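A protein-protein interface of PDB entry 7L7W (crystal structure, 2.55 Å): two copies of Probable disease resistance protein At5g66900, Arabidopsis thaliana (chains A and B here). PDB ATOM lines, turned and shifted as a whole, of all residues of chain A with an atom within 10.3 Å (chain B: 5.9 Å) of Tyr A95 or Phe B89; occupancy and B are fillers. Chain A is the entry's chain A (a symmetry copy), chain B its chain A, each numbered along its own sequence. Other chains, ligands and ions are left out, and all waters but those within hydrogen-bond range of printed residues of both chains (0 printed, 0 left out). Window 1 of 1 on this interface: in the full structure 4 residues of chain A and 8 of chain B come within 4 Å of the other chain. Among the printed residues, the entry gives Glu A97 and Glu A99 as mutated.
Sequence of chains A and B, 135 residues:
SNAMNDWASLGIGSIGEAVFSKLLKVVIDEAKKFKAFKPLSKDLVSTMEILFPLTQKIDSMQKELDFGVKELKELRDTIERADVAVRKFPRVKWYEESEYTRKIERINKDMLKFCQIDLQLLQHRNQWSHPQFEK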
ATOM      1  N   PHE A  89      22.882  -5.915 -13.536  1.00  0.00           N
ATOM      2  CA  PHE A  89      22.698  -7.224 -14.177  1.00  0.00           C
ATOM      3  C   PHE A  89      22.607  -8.413 -13.225  1.00  0.00           C
ATOM      4  O   PHE A  89      21.719  -9.264 -13.436  1.00  0.00           O
ATOM      5  CB  PHE A  89      23.810  -7.513 -15.192  1.00  0.00           C
ATOM      6  CG  PHE A  89      23.629  -8.813 -15.910  1.00  0.00           C
ATOM      7  CD1 PHE A  89      22.496  -9.033 -16.685  1.00  0.00           C
ATOM      8  CD2 PHE A  89      24.566  -9.825 -15.786  1.00  0.00           C
ATOM      9  CE1 PHE A  89      22.310 -10.235 -17.349  1.00  0.00           C
ATOM     10  CE2 PHE A  89      24.382 -11.041 -16.445  1.00  0.00           C
ATOM     11  CZ  PHE A  89      23.250 -11.243 -17.225  1.00  0.00           C
ATOM     12  N   ARG A  91      21.172  -8.858 -10.579  1.00  0.00           N
ATOM     13  CA  ARG A  91      19.839  -9.007 -10.017  1.00  0.00           C
ATOM     14  C   ARG A  91      18.742  -8.964 -11.073  1.00  0.00           C
ATOM     15  O   ARG A  91      17.566  -8.899 -10.721  1.00  0.00           O
ATOM     16  CB  ARG A  91      19.606  -7.960  -8.931  1.00  0.00           C
ATOM     17  CG  ARG A  91      20.661  -8.038  -7.823  1.00  0.00           C
ATOM     18  CD  ARG A  91      20.595  -6.853  -6.879  1.00  0.00           C
ATOM     19  NE  ARG A  91      19.660  -5.831  -7.354  1.00  0.00           N
ATOM     20  CZ  ARG A  91      19.990  -4.626  -7.835  1.00  0.00           C
ATOM     21  NH1 ARG A  91      21.265  -4.234  -7.927  1.00  0.00           N
ATOM     22  NH2 ARG A  91      19.020  -3.799  -8.227  1.00  0.00           N
ATOM     23  N   VAL A  92      19.084  -9.050 -12.356  1.00  0.00           N
ATOM     24  CA  VAL A  92      18.055  -9.235 -13.377  1.00  0.00           C
ATOM     25  C   VAL A  92      17.491 -10.654 -13.241  1.00  0.00           C
ATOM     26  O   VAL A  92      18.219 -11.641 -13.393  1.00  0.00           O
ATOM     27  CB  VAL A  92      18.616  -8.987 -14.778  1.00  0.00           C
ATOM     28  CG1 VAL A  92      17.539  -9.154 -15.811  1.00  0.00           C
ATOM     29  CG2 VAL A  92      19.178  -7.605 -14.856  1.00  0.00           C
ATOM     30  N   LYS A  93      16.198 -10.759 -12.931  1.00  0.00           N
ATOM     31  CA  LYS A  93      15.519 -12.048 -12.841  1.00  0.00           C
ATOM     32  C   LYS A  93      15.324 -12.628 -14.240  1.00  0.00           C
ATOM     33  O   LYS A  93      15.357 -11.896 -15.241  1.00  0.00           O
ATOM     34  CB  LYS A  93      14.180 -11.883 -12.117  1.00  0.00           C
ATOM     35  CG  LYS A  93      14.336 -11.078 -10.843  1.00  0.00           C
ATOM     36  CD  LYS A  93      13.096 -11.051  -9.992  1.00  0.00           C
ATOM     37  CE  LYS A  93      13.227  -9.951  -8.942  1.00  0.00           C
ATOM     38  NZ  LYS A  93      13.092  -8.559  -9.538  1.00  0.00           N
ATOM     39  N   TRP A  94      15.139 -13.958 -14.312  1.00  0.00           N
ATOM     40  CA  TRP A  94      15.155 -14.628 -15.618  1.00  0.00           C
ATOM     41  C   TRP A  94      14.034 -14.118 -16.525  1.00  0.00           C
ATOM     42  O   TRP A  94      14.218 -13.978 -17.742  1.00  0.00           O
ATOM     43  CB  TRP A  94      15.073 -16.159 -15.459  1.00  0.00           C
ATOM     44  CG  TRP A  94      13.826 -16.668 -14.756  1.00  0.00           C
ATOM     45  CD1 TRP A  94      13.698 -16.952 -13.422  1.00  0.00           C
ATOM     46  CD2 TRP A  94      12.542 -16.939 -15.348  1.00  0.00           C
ATOM     47  NE1 TRP A  94      12.417 -17.378 -13.147  1.00  0.00           N
ATOM     48  CE2 TRP A  94      11.682 -17.368 -14.305  1.00  0.00           C
ATOM     49  CE3 TRP A  94      12.031 -16.850 -16.652  1.00  0.00           C
ATOM     50  CZ2 TRP A  94      10.339 -17.714 -14.526  1.00  0.00           C
ATOM     51  CZ3 TRP A  94      10.680 -17.186 -16.870  1.00  0.00           C
ATOM     52  CH2 TRP A  94       9.860 -17.611 -15.810  1.00  0.00           C
ATOM     53  N   TYR A  95      12.876 -13.803 -15.956  1.00  0.00           N
ATOM     54  CA  TYR A  95      11.757 -13.390 -16.793  1.00  0.00           C
ATOM     55  C   TYR A  95      11.871 -11.934 -17.231  1.00  0.00           C
ATOM     56  O   TYR A  95      11.032 -11.470 -18.005  1.00  0.00           O
ATOM     57  CB  TYR A  95      10.423 -13.644 -16.068  1.00  0.00           C
ATOM     58  CG  TYR A  95      10.240 -12.877 -14.770  1.00  0.00           C
ATOM     59  CD1 TYR A  95       9.727 -11.583 -14.773  1.00  0.00           C
ATOM     60  CD2 TYR A  95      10.572 -13.444 -13.544  1.00  0.00           C
ATOM     61  CE1 TYR A  95       9.557 -10.867 -13.595  1.00  0.00           C
ATOM     62  CE2 TYR A  95      10.406 -12.742 -12.354  1.00  0.00           C
ATOM     63  CZ  TYR A  95       9.897 -11.451 -12.391  1.00  0.00           C
ATOM     64  OH  TYR A  95       9.728 -10.725 -11.235  1.00  0.00           O
ATOM     65  N   GLU A  96      12.887 -11.212 -16.771  1.00  0.00           N
ATOM     66  CA  GLU A  96      13.224  -9.897 -17.304  1.00  0.00           C
ATOM     67  C   GLU A  96      14.240  -9.952 -18.453  1.00  0.00           C
ATOM     68  O   GLU A  96      14.591  -8.891 -18.998  1.00  0.00           O
ATOM     69  CB  GLU A  96      13.744  -8.998 -16.168  1.00  0.00           C
ATOM     70  CG  GLU A  96      12.785  -8.927 -14.970  1.00  0.00           C
ATOM     71  CD  GLU A  96      13.348  -8.218 -13.724  1.00  0.00           C
ATOM     72  OE1 GLU A  96      14.497  -8.500 -13.309  1.00  0.00           O
ATOM     73  OE2 GLU A  96      12.620  -7.403 -13.117  1.00  0.00           O
ATOM     74  N   GLU A  97      14.674 -11.149 -18.879  1.00  0.00           N
ATOM     75  CA  GLU A  97      15.729 -11.213 -19.896  1.00  0.00           C
ATOM     76  C   GLU A  97      15.420 -10.336 -21.112  1.00  0.00           C
ATOM     77  O   GLU A  97      16.139  -9.367 -21.380  1.00  0.00           O
ATOM     78  CB  GLU A  97      15.974 -12.654 -20.330  1.00  0.00           C
ATOM     79  CG  GLU A  97      16.718 -12.768 -21.654  1.00  0.00           C
ATOM     80  CD  GLU A  97      17.301 -14.154 -21.874  1.00  0.00           C
ATOM     81  OE1 GLU A  97      16.645 -15.171 -21.490  1.00  0.00           O
ATOM     82  OE2 GLU A  97      18.423 -14.212 -22.427  1.00  0.00           O
ATOM     83  N   SER A  98      14.355 -10.659 -21.859  1.00  0.00           N
ATOM     84  CA  SER A  98      13.995  -9.871 -23.042  1.00  0.00           C
ATOM     85  C   SER A  98      13.999  -8.383 -22.726  1.00  0.00           C
ATOM     86  O   SER A  98      14.640  -7.581 -23.418  1.00  0.00           O
ATOM     87  CB  SER A  98      12.620 -10.281 -23.572  1.00  0.00           C
ATOM     88  OG  SER A  98      12.403 -11.673 -23.423  1.00  0.00           O
ATOM     89  N   GLU A  99      13.330  -8.004 -21.641  1.00  0.00           N
ATOM     90  CA  GLU A  99      13.261  -6.600 -21.270  1.00  0.00           C
ATOM     91  C   GLU A  99      14.652  -5.998 -21.212  1.00  0.00           C
ATOM     92  O   GLU A  99      14.983  -5.049 -21.940  1.00  0.00           O
ATOM     93  CB  GLU A  99      12.585  -6.481 -19.914  1.00  0.00           C
ATOM     94  CG  GLU A  99      12.000  -5.152 -19.624  1.00  0.00           C
ATOM     95  CD  GLU A  99      11.335  -5.140 -18.270  1.00  0.00           C
ATOM     96  OE1 GLU A  99      12.081  -5.127 -17.257  1.00  0.00           O
ATOM     97  OE2 GLU A  99      10.076  -5.175 -18.226  1.00  0.00           O
ATOM     98  N   TYR A 100      15.494  -6.592 -20.368  1.00  0.00           N
ATOM     99  CA  TYR A 100      16.820  -6.047 -20.147  1.00  0.00           C
ATOM    100  C   TYR A 100      17.605  -6.058 -21.442  1.00  0.00           C
ATOM    101  O   TYR A 100      18.289  -5.079 -21.772  1.00  0.00           O
ATOM    102  CB  TYR A 100      17.519  -6.848 -19.061  1.00  0.00           C
ATOM    103  CG  TYR A 100      18.933  -6.452 -18.738  1.00  0.00           C
ATOM    104  CD1 TYR A 100      19.201  -5.441 -17.826  1.00  0.00           C
ATOM    105  CD2 TYR A 100      20.014  -7.132 -19.304  1.00  0.00           C
ATOM    106  CE1 TYR A 100      20.509  -5.099 -17.511  1.00  0.00           C
ATOM    107  CE2 TYR A 100      21.309  -6.803 -18.993  1.00  0.00           C
ATOM    108  CZ  TYR A 100      21.561  -5.789 -18.098  1.00  0.00           C
ATOM    109  OH  TYR A 100      22.869  -5.458 -17.791  1.00  0.00           O
ATOM    110  N   THR A 101      17.433  -7.107 -22.248  1.00  0.00           N
ATOM    111  CA  THR A 101      18.221  -7.156 -23.463  1.00  0.00           C
ATOM    112  C   THR A 101      17.869  -5.987 -24.370  1.00  0.00           C
ATOM    113  O   THR A 101      18.769  -5.308 -24.880  1.00  0.00           O
ATOM    114  CB  THR A 101      18.039  -8.492 -24.158  1.00  0.00           C
ATOM    115  OG1 THR A 101      18.475  -9.526 -23.270  1.00  0.00           O
ATOM    116  CG2 THR A 101      18.908  -8.550 -25.401  1.00  0.00           C
ATOM    117  N   ARG A 102      16.572  -5.669 -24.487  1.00  0.00           N
ATOM    118  CA  ARG A 102      16.169  -4.529 -25.307  1.00  0.00           C
ATOM    119  C   ARG A 102      16.848  -3.260 -24.815  1.00  0.00           C
ATOM    120  O   ARG A 102      17.462  -2.528 -25.604  1.00  0.00           O
ATOM    121  CB  ARG A 102      14.641  -4.371 -25.308  1.00  0.00           C
ATOM    122  CG  ARG A 102      13.874  -5.495 -26.028  1.00  0.00           C
ATOM    123  CD  ARG A 102      14.697  -6.137 -27.164  1.00  0.00           C
ATOM    124  NE  ARG A 102      14.214  -7.472 -27.541  1.00  0.00           N
ATOM    125  CZ  ARG A 102      14.764  -8.614 -27.133  1.00  0.00           C
ATOM    126  NH1 ARG A 102      15.822  -8.582 -26.341  1.00  0.00           N
ATOM    127  NH2 ARG A 102      14.264  -9.789 -27.514  1.00  0.00           N
ATOM    128  N   PHE B  34       3.670  -8.406 -12.205  1.00  0.00           N
ATOM    129  CA  PHE B  34       4.766  -9.048 -12.947  1.00  0.00           C
ATOM    130  C   PHE B  34       4.747  -8.625 -14.420  1.00  0.00           C
ATOM    131  O   PHE B  34       4.593  -9.445 -15.334  1.00  0.00           O
ATOM    132  CB  PHE B  34       4.682 -10.572 -12.798  1.00  0.00           C
ATOM    133  CG  PHE B  34       4.715 -11.044 -11.362  1.00  0.00           C
ATOM    134  CD1 PHE B  34       5.849 -10.861 -10.577  1.00  0.00           C
ATOM    135  CD2 PHE B  34       3.622 -11.667 -10.797  1.00  0.00           C
ATOM    136  CE1 PHE B  34       5.872 -11.283  -9.242  1.00  0.00           C
ATOM    137  CE2 PHE B  34       3.643 -12.097  -9.461  1.00  0.00           C
ATOM    138  CZ  PHE B  34       4.759 -11.898  -8.682  1.00  0.00           C
ATOM    139  N   ALA B  36       6.965  -7.762 -16.543  1.00  0.00           N
ATOM    140  CA  ALA B  36       7.944  -8.346 -17.459  1.00  0.00           C
ATOM    141  C   ALA B  36       7.504  -9.700 -17.997  1.00  0.00           C
ATOM    142  O   ALA B  36       7.851 -10.047 -19.132  1.00  0.00           O
ATOM    143  CB  ALA B  36       9.304  -8.476 -16.781  1.00  0.00           C
ATOM    144  N   PHE B  37       6.718 -10.465 -17.221  1.00  0.00           N
ATOM    145  CA  PHE B  37       6.335 -11.841 -17.568  1.00  0.00           C
ATOM    146  C   PHE B  37       4.933 -11.814 -18.166  1.00  0.00           C
ATOM    147  O   PHE B  37       3.937 -11.688 -17.448  1.00  0.00           O
ATOM    148  CB  PHE B  37       6.413 -12.757 -16.346  1.00  0.00           C
ATOM    149  CG  PHE B  37       6.218 -14.222 -16.666  1.00  0.00           C
ATOM    150  CD1 PHE B  37       7.137 -14.905 -17.458  1.00  0.00           C
ATOM    151  CD2 PHE B  37       5.099 -14.920 -16.182  1.00  0.00           C
ATOM    152  CE1 PHE B  37       6.947 -16.254 -17.756  1.00  0.00           C
ATOM    153  CE2 PHE B  37       4.913 -16.264 -16.477  1.00  0.00           C
ATOM    154  CZ  PHE B  37       5.832 -16.931 -17.266  1.00  0.00           C
ATOM    155  N   LEU B  40       1.527 -13.975 -17.465  1.00  0.00           N
ATOM    156  CA  LEU B  40       0.771 -13.507 -16.314  1.00  0.00           C
ATOM    157  C   LEU B  40       0.124 -12.150 -16.588  1.00  0.00           C
ATOM    158  O   LEU B  40      -1.107 -12.037 -16.623  1.00  0.00           O
ATOM    159  CB  LEU B  40       1.680 -13.438 -15.083  1.00  0.00           C
ATOM    160  CG  LEU B  40       1.771 -14.723 -14.254  1.00  0.00           C
ATOM    161  CD1 LEU B  40       2.589 -14.489 -12.999  1.00  0.00           C
ATOM    162  CD2 LEU B  40       0.377 -15.263 -13.891  1.00  0.00           C
ATOM    163  N   VAL B  84      -3.061 -19.532  -6.355  1.00  0.00           N
ATOM    164  CA  VAL B  84      -1.888 -20.279  -5.914  1.00  0.00           C
ATOM    165  C   VAL B  84      -0.724 -20.077  -6.876  1.00  0.00           C
ATOM    166  O   VAL B  84       0.428 -19.863  -6.454  1.00  0.00           O
ATOM    167  CB  VAL B  84      -2.251 -21.764  -5.765  1.00  0.00           C
ATOM    168  CG1 VAL B  84      -1.011 -22.616  -5.739  1.00  0.00           C
ATOM    169  CG2 VAL B  84      -3.079 -21.969  -4.504  1.00  0.00           C
ATOM    170  N   ALA B  85      -1.002 -20.143  -8.186  1.00  0.00           N
ATOM    171  CA  ALA B  85       0.054 -19.989  -9.179  1.00  0.00           C
ATOM    172  C   ALA B  85       0.687 -18.605  -9.094  1.00  0.00           C
ATOM    173  O   ALA B  85       1.922 -18.465  -9.129  1.00  0.00           O
ATOM    174  CB  ALA B  85      -0.510 -20.250 -10.577  1.00  0.00           C
ATOM    175  N   VAL B  86      -0.144 -17.571  -8.953  1.00  0.00           N
ATOM    176  CA  VAL B  86       0.380 -16.214  -8.863  1.00  0.00           C
ATOM    177  C   VAL B  86       1.233 -16.055  -7.617  1.00  0.00           C
ATOM    178  O   VAL B  86       2.287 -15.408  -7.645  1.00  0.00           O
ATOM    179  CB  VAL B  86      -0.776 -15.199  -8.890  1.00  0.00           C
ATOM    180  CG1 VAL B  86      -0.355 -13.903  -8.234  1.00  0.00           C
ATOM    181  CG2 VAL B  86      -1.217 -14.949 -10.317  1.00  0.00           C
ATOM    182  N   ARG B  87       0.797 -16.634  -6.498  1.00  0.00           N
ATOM    183  CA  ARG B  87       1.568 -16.424  -5.283  1.00  0.00           C
ATOM    184  C   ARG B  87       2.873 -17.198  -5.300  1.00  0.00           C
ATOM    185  O   ARG B  87       3.806 -16.807  -4.593  1.00  0.00           O
ATOM    186  CB  ARG B  87       0.733 -16.766  -4.054  1.00  0.00           C
ATOM    187  CG  ARG B  87      -0.629 -16.104  -4.111  1.00  0.00           C
ATOM    188  CD  ARG B  87      -1.123 -15.657  -2.766  1.00  0.00           C
ATOM    189  NE  ARG B  87      -0.820 -14.254  -2.509  1.00  0.00           N
ATOM    190  CZ  ARG B  87      -1.739 -13.303  -2.372  1.00  0.00           C
ATOM    191  NH1 ARG B  87      -1.376 -12.050  -2.133  1.00  0.00           N
ATOM    192  NH2 ARG B  87      -3.021 -13.603  -2.470  1.00  0.00           N
ATOM    193  N   LYS B  88       2.973 -18.261  -6.114  1.00  0.00           N
ATOM    194  CA  LYS B  88       4.229 -19.004  -6.151  1.00  0.00           C
ATOM    195  C   LYS B  88       5.178 -18.494  -7.241  1.00  0.00           C
ATOM    196  O   LYS B  88       6.348 -18.886  -7.260  1.00  0.00           O
ATOM    197  CB  LYS B  88       3.973 -20.492  -6.383  1.00  0.00           C
ATOM    198  CG  LYS B  88       3.594 -20.790  -7.827  1.00  0.00           C
ATOM    199  CD  LYS B  88       3.858 -22.245  -8.285  1.00  0.00           C
ATOM    200  CE  LYS B  88       3.342 -23.284  -7.314  1.00  0.00           C
ATOM    201  NZ  LYS B  88       2.749 -24.370  -8.143  1.00  0.00           N
ATOM    202  N   PHE B  89       4.708 -17.653  -8.166  1.00  0.00           N
ATOM    203  CA  PHE B  89       5.575 -17.214  -9.267  1.00  0.00           C
ATOM    204  C   PHE B  89       6.954 -16.708  -8.855  1.00  0.00           C
ATOM    205  O   PHE B  89       7.940 -17.095  -9.515  1.00  0.00           O
ATOM    206  CB  PHE B  89       4.902 -16.126 -10.112  1.00  0.00           C
ATOM    207  CG  PHE B  89       5.729 -15.692 -11.280  1.00  0.00           C
ATOM    208  CD1 PHE B  89       6.090 -16.608 -12.263  1.00  0.00           C
ATOM    209  CD2 PHE B  89       6.176 -14.387 -11.383  1.00  0.00           C
ATOM    210  CE1 PHE B  89       6.862 -16.222 -13.347  1.00  0.00           C
ATOM    211  CE2 PHE B  89       6.961 -13.992 -12.468  1.00  0.00           C
ATOM    212  CZ  PHE B  89       7.305 -14.916 -13.447  1.00  0.00           C
ATOM    213  N   PRO B  90       7.115 -15.856  -7.840  1.00  0.00           N
ATOM    214  CA  PRO B  90       8.463 -15.378  -7.487  1.00  0.00           C
ATOM    215  C   PRO B  90       9.466 -16.485  -7.180  1.00  0.00           C
ATOM    216  O   PRO B  90      10.680 -16.242  -7.246  1.00  0.00           O
ATOM    217  CB  PRO B  90       8.210 -14.505  -6.256  1.00  0.00           C
ATOM    218  CG  PRO B  90       6.834 -13.977  -6.484  1.00  0.00           C
ATOM    219  CD  PRO B  90       6.074 -15.129  -7.085  1.00  0.00           C
ATOM    220  N   ARG B  91       9.021 -17.690  -6.850  1.00  0.00           N
ATOM    221  CA  ARG B  91       9.956 -18.779  -6.619  1.00  0.00           C
ATOM    222  C   ARG B  91       9.975 -19.795  -7.754  1.00  0.00           C
ATOM    223  O   ARG B  91      10.585 -20.853  -7.609  1.00  0.00           O
ATOM    224  CB  ARG B  91       9.664 -19.449  -5.279  1.00  0.00           C
ATOM    225  CG  ARG B  91       9.713 -18.452  -4.116  1.00  0.00           C
ATOM    226  CD  ARG B  91       9.178 -19.044  -2.826  1.00  0.00           C
ATOM    227  NE  ARG B  91       8.580 -20.364  -3.040  1.00  0.00           N
ATOM    228  CZ  ARG B  91       7.275 -20.655  -2.976  1.00  0.00           C
ATOM    229  NH1 ARG B  91       6.362 -19.718  -2.697  1.00  0.00           N
ATOM    230  NH2 ARG B  91       6.882 -21.911  -3.192  1.00  0.00           N
ATOM    231  N   VAL B  92       9.371 -19.489  -8.899  1.00  0.00           N
ATOM    232  CA  VAL B  92       9.557 -20.336 -10.074  1.00  0.00           C
ATOM    233  C   VAL B  92      10.995 -20.159 -10.573  1.00  0.00           C
ATOM    234  O   VAL B  92      11.402 -19.056 -10.954  1.00  0.00           O
ATOM    235  CB  VAL B  92       8.541 -19.997 -11.166  1.00  0.00           C
ATOM    236  CG1 VAL B  92       8.728 -20.895 -12.355  1.00  0.00           C
ATOM    237  CG2 VAL B  92       7.156 -20.156 -10.629  1.00  0.00           C
ATOM    238  N   LYS B  93      11.776 -21.240 -10.550  1.00  0.00           N
ATOM    239  CA  LYS B  93      13.144 -21.229 -11.061  1.00  0.00           C
ATOM    240  C   LYS B  93      13.122 -21.165 -12.587  1.00  0.00           C
ATOM    241  O   LYS B  93      12.115 -21.509 -13.223  1.00  0.00           O
ATOM    242  CB  LYS B  93      13.896 -22.466 -10.568  1.00  0.00           C
ATOM    243  CG  LYS B  93      13.703 -22.674  -9.079  1.00  0.00           C
ATOM    244  CD  LYS B  93      14.574 -23.757  -8.504  1.00  0.00           C
ATOM    245  CE  LYS B  93      14.065 -24.131  -7.115  1.00  0.00           C
ATOM    246  NZ  LYS B  93      12.767 -24.924  -7.165  1.00  0.00           N
ATOM    247  N   TYR B 100       5.724 -24.030 -15.913  1.00  0.00           N
ATOM    248  CA  TYR B 100       4.793 -23.113 -15.283  1.00  0.00           C
ATOM    249  C   TYR B 100       3.929 -22.451 -16.335  1.00  0.00           C
ATOM    250  O   TYR B 100       2.711 -22.320 -16.157  1.00  0.00           O
ATOM    251  CB  TYR B 100       5.568 -22.090 -14.470  1.00  0.00           C
ATOM    252  CG  TYR B 100       4.759 -21.022 -13.786  1.00  0.00           C
ATOM    253  CD1 TYR B 100       4.204 -21.238 -12.533  1.00  0.00           C
ATOM    254  CD2 TYR B 100       4.597 -19.764 -14.371  1.00  0.00           C
ATOM    255  CE1 TYR B 100       3.482 -20.238 -11.896  1.00  0.00           C
ATOM    256  CE2 TYR B 100       3.889 -18.769 -13.744  1.00  0.00           C
ATOM    257  CZ  TYR B 100       3.332 -19.002 -12.508  1.00  0.00           C
ATOM    258  OH  TYR B 100       2.615 -17.996 -11.882  1.00  0.00           O
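The side-chain carboxylate of Glu A96 lies within salt-bridge range of the side-chain amino group of Lys A93, 3.8 Å away.
Of chain B, only Phe B34, Ala B36, Phe B37 and Phe B89 come within 4 Å of Tyr A95. Printed residues of chain B within 4 Å of Glu A96: Ala B36 (3.9 Å). Of the printed residues of chain B, Glu A99 touches Ala B36 (3.7 Å). Ala B36 touches just these residues of chain A: Tyr A95, Glu A96 and Glu A99. Phe B37 touches two residues of chain A. No residue of chain A comes within 4 Å of Val B86. Phe B89 touches just these residues of chain A: Trp A94 and Tyr A95. The nearest printed residue of chain B that does not touch Tyr A95 is Pro B90 (5.9 Å). The nearest printed residue of chain A that does not touch Lys B93 is Tyr A95 (8.1 Å).
The backbone carbonyl oxygen (O) of Val B92 is in hydrogen-bond range of the indole nitrogen (NE1) of Trp A94 (2.9 Å).
Hydrophobic or aromatic side chains of chain B that line the printed part of chain A: Phe B34, Ala B36, Phe B37 and Phe B89. Of the 13 printed residues of chain A, 4 touch a printed residue of chain B. Printed residues of chain A that touch a printed residue of chain B: Trp A94, Tyr A95, Glu A96 and Glu A99. Hydrophobic or aromatic side chains of chain A that line the printed part of chain B: Trp A94 and Tyr A95. Among the printed residues, 10 pairs touch across the chains.
5 positions are printed for both chains. Of the 10 pairs that touch across the chains among the printed residues, none has its exchanged pair printed and touching as well.
CH2 of Trp A94 touches CE1 of Phe B37 (3.8 Å). CE1 of Phe B89 touches CZ2 of Trp A94, 3.96 Å away. Lys B93 touches Trp A94. Tyr A95 touches Phe B34 (OH to CD1, 3.9 Å). Tyr A95 touches Ala B36 (O to O, 3.7 Å). CD1 of Phe B37 touches CB of Tyr A95, 3.8 Å away. Tyr A95 touches Phe B89. Glu A96 touches Ala B36 (CG to CB, 3.9 Å). Glu A99 touches Ala B36 (OE2 to CB, 3.7 Å).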
